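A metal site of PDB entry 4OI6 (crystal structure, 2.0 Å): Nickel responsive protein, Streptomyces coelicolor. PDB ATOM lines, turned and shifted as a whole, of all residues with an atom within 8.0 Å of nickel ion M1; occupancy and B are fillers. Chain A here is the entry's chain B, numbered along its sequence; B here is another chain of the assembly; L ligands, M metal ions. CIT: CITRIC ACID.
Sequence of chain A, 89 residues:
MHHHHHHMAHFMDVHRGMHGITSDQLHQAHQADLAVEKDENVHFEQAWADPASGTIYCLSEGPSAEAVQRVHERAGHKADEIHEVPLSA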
ATOM      1  N   ALA A  49      18.593  -5.213 -30.730  1.00  0.00           N
ATOM      2  CA  ALA A  49      19.139  -3.860 -30.549  1.00  0.00           C
ATOM      3  C   ALA A  49      18.083  -2.772 -30.716  1.00  0.00           C
ATOM      4  O   ALA A  49      17.172  -2.890 -31.514  1.00  0.00           O
ATOM      5  CB  ALA A  49      20.313  -3.629 -31.497  1.00  0.00           C
ATOM      6  N   ASP A  50      18.242  -1.711 -29.923  1.00  0.00           N
ATOM      7  CA  ASP A  50      17.433  -0.506 -30.028  1.00  0.00           C
ATOM      8  C   ASP A  50      18.410   0.587 -30.429  1.00  0.00           C
ATOM      9  O   ASP A  50      19.093   1.173 -29.575  1.00  0.00           O
ATOM     10  CB  ASP A  50      16.744  -0.232 -28.675  1.00  0.00           C
ATOM     11  CG  ASP A  50      16.166   1.172 -28.545  1.00  0.00           C
ATOM     12  OD1 ASP A  50      16.043   1.920 -29.533  1.00  0.00           O
ATOM     13  OD2 ASP A  50      15.827   1.534 -27.400  1.00  0.00           O
ATOM     14  N   PRO A  51      18.524   0.848 -31.737  1.00  0.00           N
ATOM     15  CA  PRO A  51      19.512   1.769 -32.292  1.00  0.00           C
ATOM     16  C   PRO A  51      19.246   3.216 -31.879  1.00  0.00           C
ATOM     17  O   PRO A  51      20.170   4.025 -31.858  1.00  0.00           O
ATOM     18  CB  PRO A  51      19.318   1.620 -33.804  1.00  0.00           C
ATOM     19  CG  PRO A  51      18.643   0.306 -33.989  1.00  0.00           C
ATOM     20  CD  PRO A  51      17.742   0.182 -32.796  1.00  0.00           C
ATOM     21  N   ALA A  52      17.986   3.535 -31.569  1.00  0.00           N
ATOM     22  CA  ALA A  52      17.630   4.895 -31.176  1.00  0.00           C
ATOM     23  C   ALA A  52      18.197   5.222 -29.800  1.00  0.00           C
ATOM     24  O   ALA A  52      18.836   6.258 -29.610  1.00  0.00           O
ATOM     25  CB  ALA A  52      16.116   5.094 -31.213  1.00  0.00           C
ATOM     26  N   SER A  53      17.966   4.339 -28.838  1.00  0.00           N
ATOM     27  CA  SER A  53      18.572   4.480 -27.512  1.00  0.00           C
ATOM     28  C   SER A  53      20.059   4.094 -27.552  1.00  0.00           C
ATOM     29  O   SER A  53      20.850   4.531 -26.696  1.00  0.00           O
ATOM     30  CB  SER A  53      17.861   3.590 -26.475  1.00  0.00           C
ATOM     31  OG  SER A  53      16.528   4.035 -26.215  1.00  0.00           O
ATOM     32  N   GLY A  54      20.425   3.280 -28.539  1.00  0.00           N
ATOM     33  CA  GLY A  54      21.805   2.816 -28.669  1.00  0.00           C
ATOM     34  C   GLY A  54      22.128   1.634 -27.762  1.00  0.00           C
ATOM     35  O   GLY A  54      23.216   1.556 -27.205  1.00  0.00           O
ATOM     36  N   THR A  55      21.180   0.702 -27.626  1.00  0.00           N
ATOM     37  CA  THR A  55      21.293  -0.381 -26.656  1.00  0.00           C
ATOM     38  C   THR A  55      21.272  -1.761 -27.324  1.00  0.00           C
ATOM     39  O   THR A  55      20.482  -2.002 -28.229  1.00  0.00           O
ATOM     40  CB  THR A  55      20.155  -0.297 -25.621  1.00  0.00           C
ATOM     41  OG1 THR A  55      20.249   0.941 -24.903  1.00  0.00           O
ATOM     42  CG2 THR A  55      20.224  -1.449 -24.615  1.00  0.00           C
ATOM     43  N   TYR A  57      20.752  -5.762 -26.260  1.00  0.00           N
ATOM     44  CA  TYR A  57      20.374  -6.785 -25.287  1.00  0.00           C
ATOM     45  C   TYR A  57      20.898  -8.140 -25.775  1.00  0.00           C
ATOM     46  O   TYR A  57      20.708  -8.511 -26.931  1.00  0.00           O
ATOM     47  CB  TYR A  57      18.858  -6.852 -25.138  1.00  0.00           C
ATOM     48  CG  TYR A  57      18.199  -5.552 -24.731  1.00  0.00           C
ATOM     49  CD1 TYR A  57      17.822  -4.614 -25.681  1.00  0.00           C
ATOM     50  CD2 TYR A  57      17.944  -5.265 -23.395  1.00  0.00           C
ATOM     51  CE1 TYR A  57      17.216  -3.412 -25.307  1.00  0.00           C
ATOM     52  CE2 TYR A  57      17.338  -4.074 -22.999  1.00  0.00           C
ATOM     53  CZ  TYR A  57      16.980  -3.148 -23.959  1.00  0.00           C
ATOM     54  OH  TYR A  57      16.376  -1.963 -23.571  1.00  0.00           O
ATOM     55  N   MET B  12      11.362  -4.773 -26.039  1.00  0.00           N
ATOM     56  CA  MET B  12      11.913  -5.322 -24.815  1.00  0.00           C
ATOM     57  C   MET B  12      11.544  -4.371 -23.696  1.00  0.00           C
ATOM     58  O   MET B  12      11.856  -3.182 -23.778  1.00  0.00           O
ATOM     59  CB  MET B  12      13.435  -5.420 -24.897  1.00  0.00           C
ATOM     60  CG  MET B  12      14.070  -6.008 -23.635  1.00  0.00           C
ATOM     61  SD  MET B  12      13.841  -7.956 -23.651  1.00  0.00           S
ATOM     62  CE  MET B  12      15.334  -8.387 -24.798  1.00  0.00           C
ATOM     63  N   GLU B  81      10.372   0.394 -18.045  1.00  0.00           N
ATOM     64  CA  GLU B  81      10.876   0.860 -19.327  1.00  0.00           C
ATOM     65  C   GLU B  81      10.417  -0.043 -20.439  1.00  0.00           C
ATOM     66  O   GLU B  81      10.289  -1.240 -20.247  1.00  0.00           O
ATOM     67  CB  GLU B  81      12.410   0.879 -19.349  1.00  0.00           C
ATOM     68  CG  GLU B  81      13.038   1.815 -18.355  1.00  0.00           C
ATOM     69  CD  GLU B  81      14.505   2.023 -18.651  1.00  0.00           C
ATOM     70  OE1 GLU B  81      14.795   2.475 -19.782  1.00  0.00           O
ATOM     71  OE2 GLU B  81      15.342   1.727 -17.767  1.00  0.00           O
ATOM     72  N   ILE B  82      10.214   0.532 -21.619  1.00  0.00           N
ATOM     73  CA  ILE B  82       9.913  -0.245 -22.806  1.00  0.00           C
ATOM     74  C   ILE B  82      10.612   0.363 -24.027  1.00  0.00           C
ATOM     75  O   ILE B  82      10.502   1.562 -24.293  1.00  0.00           O
ATOM     76  CB  ILE B  82       8.393  -0.375 -23.040  1.00  0.00           C
ATOM     77  CG1 ILE B  82       8.146  -1.006 -24.403  1.00  0.00           C
ATOM     78  CG2 ILE B  82       7.690   0.980 -22.978  1.00  0.00           C
ATOM     79  CD1 ILE B  82       6.811  -1.657 -24.492  1.00  0.00           C
ATOM     80  N   HIS B  83      11.348  -0.478 -24.757  1.00  0.00           N
ATOM     81  CA  HIS B  83      12.126  -0.018 -25.907  1.00  0.00           C
ATOM     82  C   HIS B  83      11.830  -0.877 -27.121  1.00  0.00           C
ATOM     83  O   HIS B  83      11.741  -2.093 -27.005  1.00  0.00           O
ATOM     84  CB  HIS B  83      13.622  -0.112 -25.585  1.00  0.00           C
ATOM     85  CG  HIS B  83      14.062   0.786 -24.463  1.00  0.00           C
ATOM     86  ND1 HIS B  83      14.411   2.105 -24.661  1.00  0.00           N
ATOM     87  CD2 HIS B  83      14.226   0.538 -23.144  1.00  0.00           C
ATOM     88  CE1 HIS B  83      14.758   2.639 -23.502  1.00  0.00           C
ATOM     89  NE2 HIS B  83      14.663   1.715 -22.572  1.00  0.00           N
ATOM     90  N   GLU B  84      11.702  -0.267 -28.298  1.00  0.00           N
ATOM     91  CA  GLU B  84      11.531  -1.073 -29.503  1.00  0.00           C
ATOM     92  C   GLU B  84      12.889  -1.664 -29.877  1.00  0.00           C
ATOM     93  O   GLU B  84      13.901  -0.970 -29.822  1.00  0.00           O
ATOM     94  CB  GLU B  84      10.991  -0.233 -30.671  1.00  0.00           C
ATOM     95  CG  GLU B  84      10.422  -1.063 -31.833  1.00  0.00           C
ATOM     96  CD  GLU B  84       9.940  -0.201 -32.996  1.00  0.00           C
ATOM     97  OE1 GLU B  84       9.564   0.965 -32.753  1.00  0.00           O
ATOM     98  OE2 GLU B  84       9.957  -0.669 -34.150  1.00  0.00           O
ATOM     99  N   VAL B  85      12.901  -2.938 -30.252  1.00  0.00           N
ATOM    100  CA  VAL B  85      14.134  -3.568 -30.729  1.00  0.00           C
ATOM    101  C   VAL B  85      13.968  -4.022 -32.186  1.00  0.00           C
ATOM    102  O   VAL B  85      13.776  -5.196 -32.457  1.00  0.00           O
ATOM    103  CB  VAL B  85      14.576  -4.737 -29.795  1.00  0.00           C
ATOM    104  CG1 VAL B  85      15.172  -4.192 -28.500  1.00  0.00           C
ATOM    105  CG2 VAL B  85      13.398  -5.653 -29.471  1.00  0.00           C
ATOM    106  N   PRO B  86      14.074  -3.064 -33.126  1.00  0.00           N
ATOM    107  CA  PRO B  86      13.796  -3.419 -34.535  1.00  0.00           C
ATOM    108  C   PRO B  86      14.839  -4.364 -35.134  1.00  0.00           C
ATOM    109  O   PRO B  86      14.605  -4.947 -36.193  1.00  0.00           O
ATOM    110  CB  PRO B  86      13.816  -2.069 -35.259  1.00  0.00           C
ATOM    111  CG  PRO B  86      14.653  -1.158 -34.386  1.00  0.00           C
ATOM    112  CD  PRO B  86      14.514  -1.671 -32.967  1.00  0.00           C
HETATM  113  C1  CIT L   1      14.731   7.323 -28.443  1.00  0.00           C
HETATM  114  O1  CIT L   1      15.720   6.705 -27.979  1.00  0.00           O
HETATM  115  O2  CIT L   1      14.721   8.578 -28.375  1.00  0.00           O
HETATM  116  C2  CIT L   1      13.581   6.562 -29.041  1.00  0.00           C
HETATM  117  C3  CIT L   1      13.359   5.265 -28.254  1.00  0.00           C
HETATM  118  O7  CIT L   1      14.541   4.432 -28.333  1.00  0.00           O
HETATM  119  C4  CIT L   1      12.114   4.556 -28.826  1.00  0.00           C
HETATM  120  C5  CIT L   1      11.948   3.123 -28.379  1.00  0.00           C
HETATM  121  O3  CIT L   1      10.959   2.443 -28.773  1.00  0.00           O
HETATM  122  O4  CIT L   1      12.774   2.592 -27.609  1.00  0.00           O
HETATM  123  C6  CIT L   1      13.137   5.653 -26.798  1.00  0.00           C
HETATM  124  O5  CIT L   1      12.348   6.575 -26.505  1.00  0.00           O
HETATM  125  O6  CIT L   1      13.756   5.062 -25.890  1.00  0.00           O
HETATM  126 NI    NI M   1      14.594   3.145 -26.699  1.00  0.00          NI
HETATM  127 NI    NI M   2      16.841   2.368 -19.422  1.00  0.00          NI
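The side-chain carboxylate of Asp 50 sits close to the backbone NH of Ala 52 (3.2 Å). The backbone NH of Asp 50 sits at hydrogen-bond distance from the backbone carbonyl oxygen of Thr 55, at 2.8 Å. A ring nitrogen (NE2) of His 83 of chain B lies close to the side-chain carboxylate (OE1) of Glu 81 of chain B. N of Met 12 of chain B sits at hydrogen-bond distance from O of His 83 of chain B.
Within 4 Å of nickel ion M1: Asp 50, Ser 53 and His 83 of chain B. The nearest printed residue that does not touch nickel ion M1 is Glu 84 of chain B (4.7 Å).
Nickel ion M1 is bound by an oxygen (O7) of the ligand, an oxygen (O4) of the ligand, the side-chain carboxylate of Asp 50, the side-chain hydroxyl of Ser 53, an oxygen (O6) of the ligand and a ring nitrogen (ND1) of His 83 of chain B. Nickel ion M1 has six donor atoms within binding distance.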
